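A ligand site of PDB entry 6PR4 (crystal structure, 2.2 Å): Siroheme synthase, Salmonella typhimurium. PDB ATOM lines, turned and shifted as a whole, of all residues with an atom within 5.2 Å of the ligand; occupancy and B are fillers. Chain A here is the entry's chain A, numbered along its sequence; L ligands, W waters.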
ATOM      1  N   PRO A 225      -0.446  21.570  -3.110  1.00  0.00           N
ATOM      2  CA  PRO A 225      -1.660  20.755  -3.262  1.00  0.00           C
ATOM      3  C   PRO A 225      -2.560  21.128  -4.421  1.00  0.00           C
ATOM      4  O   PRO A 225      -3.645  20.557  -4.532  1.00  0.00           O
ATOM      5  CB  PRO A 225      -2.375  20.981  -1.916  1.00  0.00           C
ATOM      6  CG  PRO A 225      -1.988  22.353  -1.512  1.00  0.00           C
ATOM      7  CD  PRO A 225      -0.590  22.616  -2.080  1.00  0.00           C
ATOM      8  N   GLY A 226      -2.175  22.042  -5.315  1.00  0.00           N
ATOM      9  CA  GLY A 226      -3.074  22.393  -6.399  1.00  0.00           C
ATOM     10  C   GLY A 226      -2.935  23.799  -6.947  1.00  0.00           C
ATOM     11  O   GLY A 226      -2.519  23.973  -8.095  1.00  0.00           O
ATOM     12  N   LEU A 250      -1.727  13.902  -9.167  1.00  0.00           N
ATOM     13  CA  LEU A 250      -1.998  14.860  -8.105  1.00  0.00           C
ATOM     14  C   LEU A 250      -1.230  16.167  -8.256  1.00  0.00           C
ATOM     15  O   LEU A 250      -1.277  17.006  -7.350  1.00  0.00           O
ATOM     16  CB  LEU A 250      -1.676  14.258  -6.731  1.00  0.00           C
ATOM     17  CG  LEU A 250      -2.712  13.317  -6.117  1.00  0.00           C
ATOM     18  CD1 LEU A 250      -2.406  13.095  -4.653  1.00  0.00           C
ATOM     19  CD2 LEU A 250      -4.113  13.886  -6.296  1.00  0.00           C
ATOM     20  N   GLY A 301       2.876  15.909  -6.027  1.00  0.00           N
ATOM     21  CA  GLY A 301       1.873  16.662  -5.308  1.00  0.00           C
ATOM     22  C   GLY A 301       2.280  16.890  -3.866  1.00  0.00           C
ATOM     23  O   GLY A 301       2.915  16.040  -3.235  1.00  0.00           O
ATOM     24  N   GLY A 302       1.928  18.070  -3.367  1.00  0.00           N
ATOM     25  CA  GLY A 302       2.170  18.366  -1.963  1.00  0.00           C
ATOM     26  C   GLY A 302       3.660  18.484  -1.652  1.00  0.00           C
ATOM     27  O   GLY A 302       4.391  19.220  -2.318  1.00  0.00           O
ATOM     28  N   ASP A 303       4.090  17.781  -0.599  1.00  0.00           N
ATOM     29  CA  ASP A 303       5.483  17.698  -0.153  1.00  0.00           C
ATOM     30  C   ASP A 303       6.031  16.307  -0.438  1.00  0.00           C
ATOM     31  O   ASP A 303       5.352  15.303  -0.122  1.00  0.00           O
ATOM     32  CB  ASP A 303       5.579  18.022   1.350  1.00  0.00           C
ATOM     33  CG  ASP A 303       7.019  17.981   1.863  1.00  0.00           C
ATOM     34  OD1 ASP A 303       7.733  19.010   1.785  1.00  0.00           O
ATOM     35  OD2 ASP A 303       7.431  16.894   2.359  1.00  0.00           O
ATOM     36  N   PRO A 304       7.238  16.178  -0.997  1.00  0.00           N
ATOM     37  CA  PRO A 304       7.706  14.841  -1.428  1.00  0.00           C
ATOM     38  C   PRO A 304       7.969  13.890  -0.288  1.00  0.00           C
ATOM     39  O   PRO A 304       7.974  12.672  -0.501  1.00  0.00           O
ATOM     40  CB  PRO A 304       8.998  15.145  -2.207  1.00  0.00           C
ATOM     41  CG  PRO A 304       9.026  16.625  -2.412  1.00  0.00           C
ATOM     42  CD  PRO A 304       8.242  17.220  -1.263  1.00  0.00           C
ATOM     43  N   ILE A 306       6.243  13.542   2.660  1.00  0.00           N
ATOM     44  CA  ILE A 306       5.083  13.285   3.514  1.00  0.00           C
ATOM     45  C   ILE A 306       4.120  12.402   2.729  1.00  0.00           C
ATOM     46  O   ILE A 306       3.369  12.902   1.875  1.00  0.00           O
ATOM     47  CB  ILE A 306       4.419  14.582   3.999  1.00  0.00           C
ATOM     48  CG1 ILE A 306       5.405  15.411   4.829  1.00  0.00           C
ATOM     49  CG2 ILE A 306       3.159  14.283   4.833  1.00  0.00           C
ATOM     50  CD1 ILE A 306       4.935  16.797   5.235  1.00  0.00           C
ATOM     51  N   PHE A 307       4.160  11.090   2.994  1.00  0.00           N
ATOM     52  CA  PHE A 307       3.312  10.099   2.321  1.00  0.00           C
ATOM     53  C   PHE A 307       3.456  10.156   0.803  1.00  0.00           C
ATOM     54  O   PHE A 307       2.490   9.991   0.048  1.00  0.00           O
ATOM     55  CB  PHE A 307       1.833  10.259   2.721  1.00  0.00           C
ATOM     56  CG  PHE A 307       1.595  10.077   4.175  1.00  0.00           C
ATOM     57  CD1 PHE A 307       1.987   8.909   4.816  1.00  0.00           C
ATOM     58  CD2 PHE A 307       0.999  11.080   4.923  1.00  0.00           C
ATOM     59  CE1 PHE A 307       1.770   8.734   6.171  1.00  0.00           C
ATOM     60  CE2 PHE A 307       0.774  10.903   6.284  1.00  0.00           C
ATOM     61  CZ  PHE A 307       1.161   9.732   6.901  1.00  0.00           C
ATOM     62  N   GLY A 308       4.676  10.416   0.337  1.00  0.00           N
ATOM     63  CA  GLY A 308       4.890  10.580  -1.087  1.00  0.00           C
ATOM     64  C   GLY A 308       5.896   9.621  -1.665  1.00  0.00           C
ATOM     65  O   GLY A 308       6.276   9.770  -2.830  1.00  0.00           O
ATOM     66  N   ILE A 330       4.307  22.710  -0.082  1.00  0.00           N
ATOM     67  CA  ILE A 330       3.150  22.843   0.792  1.00  0.00           C
ATOM     68  C   ILE A 330       2.418  21.500   0.803  1.00  0.00           C
ATOM     69  O   ILE A 330       1.846  21.083  -0.204  1.00  0.00           O
ATOM     70  CB  ILE A 330       2.212  23.948   0.319  1.00  0.00           C
ATOM     71  CG1 ILE A 330       2.935  25.306   0.142  1.00  0.00           C
ATOM     72  CG2 ILE A 330       1.021  24.015   1.246  1.00  0.00           C
ATOM     73  CD1 ILE A 330       3.416  25.964   1.415  1.00  0.00           C
ATOM     74  N   THR A 331       2.432  20.816   1.947  1.00  0.00           N
ATOM     75  CA  THR A 331       1.706  19.556   2.033  1.00  0.00           C
ATOM     76  C   THR A 331       0.192  19.814   2.053  1.00  0.00           C
ATOM     77  O   THR A 331      -0.284  20.923   2.338  1.00  0.00           O
ATOM     78  CB  THR A 331       2.149  18.796   3.292  1.00  0.00           C
ATOM     79  OG1 THR A 331       1.683  17.437   3.224  1.00  0.00           O
ATOM     80  CG2 THR A 331       1.627  19.494   4.527  1.00  0.00           C
ATOM     81  N   ALA A 332      -0.572  18.775   1.690  1.00  0.00           N
ATOM     82  CA  ALA A 332      -2.017  18.937   1.563  1.00  0.00           C
ATOM     83  C   ALA A 332      -2.629  19.476   2.857  1.00  0.00           C
ATOM     84  O   ALA A 332      -3.543  20.308   2.803  1.00  0.00           O
ATOM     85  CB  ALA A 332      -2.673  17.609   1.180  1.00  0.00           C
ATOM     86  N   ALA A 333      -2.137  19.023   4.013  1.00  0.00           N
ATOM     87  CA  ALA A 333      -2.665  19.490   5.294  1.00  0.00           C
ATOM     88  C   ALA A 333      -2.551  21.009   5.423  1.00  0.00           C
ATOM     89  O   ALA A 333      -3.528  21.687   5.778  1.00  0.00           O
ATOM     90  CB  ALA A 333      -1.929  18.802   6.448  1.00  0.00           C
ATOM     91  N   CYS A 336      -4.910  22.812   2.649  1.00  0.00           N
ATOM     92  CA  CYS A 336      -6.328  22.706   2.994  1.00  0.00           C
ATOM     93  C   CYS A 336      -6.651  23.458   4.274  1.00  0.00           C
ATOM     94  O   CYS A 336      -7.712  24.105   4.378  1.00  0.00           O
ATOM     95  CB  CYS A 336      -6.732  21.240   3.115  1.00  0.00           C
ATOM     96  SG  CYS A 336      -6.674  20.338   1.544  1.00  0.00           S
ATOM     97  N   PHE A 380      -6.193  12.871   8.089  1.00  0.00           N
ATOM     98  CA  PHE A 380      -6.066  11.601   7.378  1.00  0.00           C
ATOM     99  C   PHE A 380      -5.838  11.853   5.898  1.00  0.00           C
ATOM    100  O   PHE A 380      -6.658  12.480   5.228  1.00  0.00           O
ATOM    101  CB  PHE A 380      -7.317  10.739   7.549  1.00  0.00           C
ATOM    102  CG  PHE A 380      -7.489  10.220   8.937  1.00  0.00           C
ATOM    103  CD1 PHE A 380      -6.968   8.984   9.289  1.00  0.00           C
ATOM    104  CD2 PHE A 380      -8.139  10.980   9.892  1.00  0.00           C
ATOM    105  CE1 PHE A 380      -7.110   8.512  10.582  1.00  0.00           C
ATOM    106  CE2 PHE A 380      -8.286  10.513  11.164  1.00  0.00           C
ATOM    107  CZ  PHE A 380      -7.744   9.284  11.527  1.00  0.00           C
ATOM    108  N   TYR A 381      -4.709  11.364   5.409  1.00  0.00           N
ATOM    109  CA  TYR A 381      -4.427  11.328   3.986  1.00  0.00           C
ATOM    110  C   TYR A 381      -4.950  10.013   3.433  1.00  0.00           C
ATOM    111  O   TYR A 381      -4.859   8.973   4.093  1.00  0.00           O
ATOM    112  CB  TYR A 381      -2.923  11.434   3.743  1.00  0.00           C
ATOM    113  CG  TYR A 381      -2.327  12.803   3.986  1.00  0.00           C
ATOM    114  CD1 TYR A 381      -2.352  13.404   5.255  1.00  0.00           C
ATOM    115  CD2 TYR A 381      -1.701  13.501   2.948  1.00  0.00           C
ATOM    116  CE1 TYR A 381      -1.780  14.666   5.473  1.00  0.00           C
ATOM    117  CE2 TYR A 381      -1.136  14.765   3.159  1.00  0.00           C
ATOM    118  CZ  TYR A 381      -1.170  15.336   4.426  1.00  0.00           C
ATOM    119  OH  TYR A 381      -0.603  16.588   4.605  1.00  0.00           O
ATOM    120  N   MET A 382      -5.479  10.069   2.215  1.00  0.00           N
ATOM    121  CA  MET A 382      -6.032   8.930   1.480  1.00  0.00           C
ATOM    122  C   MET A 382      -6.810   7.983   2.385  1.00  0.00           C
ATOM    123  O   MET A 382      -6.592   6.768   2.396  1.00  0.00           O
ATOM    124  CB  MET A 382      -4.931   8.193   0.692  1.00  0.00           C
ATOM    125  CG  MET A 382      -3.705   7.749   1.481  1.00  0.00           C
ATOM    126  SD  MET A 382      -2.197   7.680   0.490  1.00  0.00           S
ATOM    127  CE  MET A 382      -0.974   7.572   1.785  1.00  0.00           C
ATOM    128  N   GLY A 383      -7.712   8.569   3.169  1.00  0.00           N
ATOM    129  CA  GLY A 383      -8.566   7.820   4.080  1.00  0.00           C
ATOM    130  C   GLY A 383     -10.026   7.768   3.679  1.00  0.00           C
ATOM    131  O   GLY A 383     -10.846   7.216   4.440  1.00  0.00           O
ATOM    132  N   VAL A 408     -12.027  18.006   3.061  1.00  0.00           N
ATOM    133  CA  VAL A 408     -11.646  19.033   2.096  1.00  0.00           C
ATOM    134  C   VAL A 408     -11.270  18.313   0.807  1.00  0.00           C
ATOM    135  O   VAL A 408     -10.282  17.568   0.765  1.00  0.00           O
ATOM    136  CB  VAL A 408     -10.501  19.916   2.607  1.00  0.00           C
ATOM    137  CG1 VAL A 408     -10.233  21.043   1.594  1.00  0.00           C
ATOM    138  CG2 VAL A 408     -10.861  20.485   3.988  1.00  0.00           C
ATOM    139  N   GLU A 409     -12.081  18.502  -0.227  1.00  0.00           N
ATOM    140  CA  GLU A 409     -11.873  17.858  -1.509  1.00  0.00           C
ATOM    141  C   GLU A 409     -11.224  18.863  -2.459  1.00  0.00           C
ATOM    142  O   GLU A 409     -11.734  19.983  -2.622  1.00  0.00           O
ATOM    143  CB  GLU A 409     -13.193  17.344  -2.093  1.00  0.00           C
ATOM    144  CG  GLU A 409     -13.024  16.687  -3.440  1.00  0.00           C
ATOM    145  CD  GLU A 409     -14.324  16.305  -4.126  1.00  0.00           C
ATOM    146  OE1 GLU A 409     -15.377  16.923  -3.845  1.00  0.00           O
ATOM    147  OE2 GLU A 409     -14.286  15.386  -4.967  1.00  0.00           O
ATOM    148  N   ASN A 410     -10.090  18.478  -3.059  1.00  0.00           N
ATOM    149  CA  ASN A 410      -9.405  19.338  -4.018  1.00  0.00           C
ATOM    150  C   ASN A 410      -9.042  20.673  -3.368  1.00  0.00           C
ATOM    151  O   ASN A 410      -9.361  21.745  -3.898  1.00  0.00           O
ATOM    152  CB  ASN A 410     -10.271  19.559  -5.268  1.00  0.00           C
ATOM    153  CG  ASN A 410     -10.215  18.392  -6.228  1.00  0.00           C
ATOM    154  OD1 ASN A 410      -9.117  17.913  -6.562  1.00  0.00           O
ATOM    155  ND2 ASN A 410     -11.386  17.918  -6.672  1.00  0.00           N
ATOM    156  N   GLY A 411      -8.413  20.595  -2.193  1.00  0.00           N
ATOM    157  CA  GLY A 411      -8.120  21.798  -1.438  1.00  0.00           C
ATOM    158  C   GLY A 411      -7.175  22.730  -2.195  1.00  0.00           C
ATOM    159  O   GLY A 411      -6.271  22.277  -2.898  1.00  0.00           O
ATOM    160  N   SER A 435     -11.948  11.451  -4.000  1.00  0.00           N
ATOM    161  CA  SER A 435     -10.518  11.704  -4.091  1.00  0.00           C
ATOM    162  C   SER A 435     -10.231  12.891  -5.019  1.00  0.00           C
ATOM    163  O   SER A 435     -10.980  13.112  -5.988  1.00  0.00           O
ATOM    164  CB  SER A 435      -9.824  10.439  -4.579  1.00  0.00           C
ATOM    165  OG  SER A 435      -8.492  10.695  -5.007  1.00  0.00           O
ATOM    166  N   PRO A 436      -9.201  13.711  -4.755  1.00  0.00           N
ATOM    167  CA  PRO A 436      -8.365  13.698  -3.538  1.00  0.00           C
ATOM    168  C   PRO A 436      -9.001  14.517  -2.425  1.00  0.00           C
ATOM    169  O   PRO A 436      -9.394  15.667  -2.630  1.00  0.00           O
ATOM    170  CB  PRO A 436      -7.043  14.317  -3.999  1.00  0.00           C
ATOM    171  CG  PRO A 436      -7.443  15.265  -5.113  1.00  0.00           C
ATOM    172  CD  PRO A 436      -8.658  14.634  -5.774  1.00  0.00           C
ATOM    173  N   ALA A 437      -9.093  13.909  -1.247  1.00  0.00           N
ATOM    174  CA  ALA A 437      -9.709  14.568  -0.119  1.00  0.00           C
ATOM    175  C   ALA A 437      -8.904  14.291   1.155  1.00  0.00           C
ATOM    176  O   ALA A 437      -8.290  13.240   1.316  1.00  0.00           O
ATOM    177  CB  ALA A 437     -11.161  14.122   0.070  1.00  0.00           C
ATOM    178  N   LEU A 438      -8.905  15.283   2.026  1.00  0.00           N
ATOM    179  CA  LEU A 438      -8.358  15.182   3.366  1.00  0.00           C
ATOM    180  C   LEU A 438      -9.521  15.048   4.342  1.00  0.00           C
ATOM    181  O   LEU A 438     -10.570  15.676   4.140  1.00  0.00           O
ATOM    182  CB  LEU A 438      -7.552  16.443   3.676  1.00  0.00           C
ATOM    183  CG  LEU A 438      -6.142  16.386   4.212  1.00  0.00           C
ATOM    184  CD1 LEU A 438      -5.277  15.364   3.466  1.00  0.00           C
ATOM    185  CD2 LEU A 438      -5.579  17.790   4.109  1.00  0.00           C
HETATM  186  N1  LIG L   1       2.756  14.044  -0.726  1.00  0.00           N
HETATM  187  C1  LIG L   1       1.426  14.668  -0.664  1.00  0.00           C
HETATM  188  C2  LIG L   1       0.344  13.634  -0.380  1.00  0.00           C
HETATM  189  C3  LIG L   1       0.448  12.300  -1.118  1.00  0.00           C
HETATM  190  S1  LIG L   1      -0.724  11.054  -0.474  1.00  0.00           S
HETATM  191  C4  LIG L   1       1.313  15.790   0.390  1.00  0.00           C
HETATM  192  O1  LIG L   1       2.259  16.087   1.120  1.00  0.00           O
HETATM  193  O2  LIG L   1       0.256  16.427   0.528  1.00  0.00           O
HETATM  194  C5  LIG L   1      -2.153  11.554  -1.477  1.00  0.00           C
HETATM  195  C6  LIG L   1      -3.292  12.079  -0.596  1.00  0.00           C
HETATM  196  O3  LIG L   1      -3.051  13.428  -0.247  1.00  0.00           O
HETATM  197  C7  LIG L   1      -4.670  12.070  -1.236  1.00  0.00           C
HETATM  198  O4  LIG L   1      -5.288  10.821  -1.160  1.00  0.00           O
HETATM  199  C8  LIG L   1      -5.395  13.132  -0.424  1.00  0.00           C
HETATM  200  O5  LIG L   1      -5.847  12.650   0.827  1.00  0.00           O
HETATM  201  C9  LIG L   1      -4.277  14.098  -0.097  1.00  0.00           C
HETATM  202  N2  LIG L   1      -4.312  15.273  -0.988  1.00  0.00           N
HETATM  203  C10 LIG L   1      -3.408  15.644  -1.963  1.00  0.00           C
HETATM  204  N3  LIG L   1      -3.827  16.802  -2.528  1.00  0.00           N
HETATM  205  C11 LIG L   1      -5.006  17.147  -1.928  1.00  0.00           C
HETATM  206  C12 LIG L   1      -5.872  18.209  -2.105  1.00  0.00           C
HETATM  207  N4  LIG L   1      -5.592  19.130  -3.012  1.00  0.00           N
HETATM  208  N5  LIG L   1      -7.003  18.298  -1.337  1.00  0.00           N
HETATM  209  C13 LIG L   1      -7.288  17.337  -0.397  1.00  0.00           C
HETATM  210  N6  LIG L   1      -6.421  16.284  -0.217  1.00  0.00           N
HETATM  211  C14 LIG L   1      -5.311  16.194  -0.980  1.00  0.00           C
HETATM  212  O   HOH W   1       3.400  13.098  -3.168  1.00  0.00           O
HETATM  213  O   HOH W   2      -8.242  11.001  -1.525  1.00  0.00           O
HETATM  214  O   HOH W   3      -1.653  17.387  -4.440  1.00  0.00           O
HETATM  215  O   HOH W   4      -0.541  15.374  -3.271  1.00  0.00           O
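An oxygen (O5) of the ligand is in hydrogen-bond range of the backbone carbonyl oxygen (O) of Ala 437, at 2.6 Å. OG1 of Thr 331 lies within hydrogen-bond range of O1 of the ligand, at 2.6 Å. An oxygen (O2) of the ligand lies within hydrogen-bond range of the backbone NH of Ala 332 (2.7 Å). The backbone NH (N) of Gly 411 sits at hydrogen-bond distance from a nitrogen (N5) of the ligand, 2.8 Å away. O of Gly 411 is in hydrogen-bond range of N4 of the ligand (3.2 Å). The backbone carbonyl oxygen (O) of Pro 225 lies within hydrogen-bond range of a nitrogen (N4) of the ligand, 2.9 Å away. A nitrogen (N1) of the ligand lies within hydrogen-bond range of the backbone carbonyl oxygen (O) of Ile 306, 2.9 Å away. O1 of the ligand lies within hydrogen-bond range of N of Asp 303 (3.0 Å). A nitrogen (N1) of the ligand lies within hydrogen-bond range of the backbone carbonyl oxygen of Asp 303, at 2.9 Å. N of Met 382 lies within hydrogen-bond range of O5 of the ligand (3.0 Å). O of Gly 301 is in hydrogen-bond range of N1 of the ligand (3.2 Å). The backbone NH of Leu 438 sits at hydrogen-bond distance from a nitrogen (N6) of the ligand (3.5 Å). The side-chain sulfur (SG) of Cys 336 is in hydrogen-bond range of a nitrogen (N5) of the ligand (3.5 Å).
The side-chain hydroxyl (OG1) of Thr 331 is in hydrogen-bond range of the side-chain hydroxyl (OH) of Tyr 381, 2.8 Å away. SG of Cys 336 sits close to O of Ala 332 (3.4 Å). O of Val 408 lies within hydrogen-bond range of N of Leu 438, 3.0 Å away. OH of Tyr 381 lies within hydrogen-bond range of N of Ala 333 (2.9 Å). O of Pro 436 sits at hydrogen-bond distance from N of Asn 410, at 2.9 Å.
The backbone carbonyl oxygen (O) of Phe 307 sits close to a sulfur (S1) of the ligand. Leu 250 touches the ligand (CD1 to C5, 3.5 Å). CA of Gly 302 touches C4 of the ligand, at 3.6 Å. Tyr 381 touches the ligand (CE2 to O2, 3.4 Å). Val 408 touches the ligand. Asn 410 touches the ligand (N to N5, 3.5 Å). Pro 436 touches the ligand (O to C13, 3.5 Å). Hydrophobic or aromatic side chains that line the ligand: Pro 225, Leu 250, Ile 306, Ala 332, Tyr 381, Met 382, Pro 436 and Leu 438. Of the 27 residues printed, 18 come within 4 Å of the ligand. The nearest printed residue that does not touch the ligand is Gly 308 (4.1 Å).
Water W1 bridges a nitrogen (N1) of the ligand (2.7 Å) and the backbone carbonyl oxygen of Gly 301 (3.0 Å). Water W3 bridges N3 of the ligand and O of Leu 250. Water W2 lies within hydrogen-bond range of O4 of the ligand (3.0 Å) and N of Ala 437 (3.0 Å).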
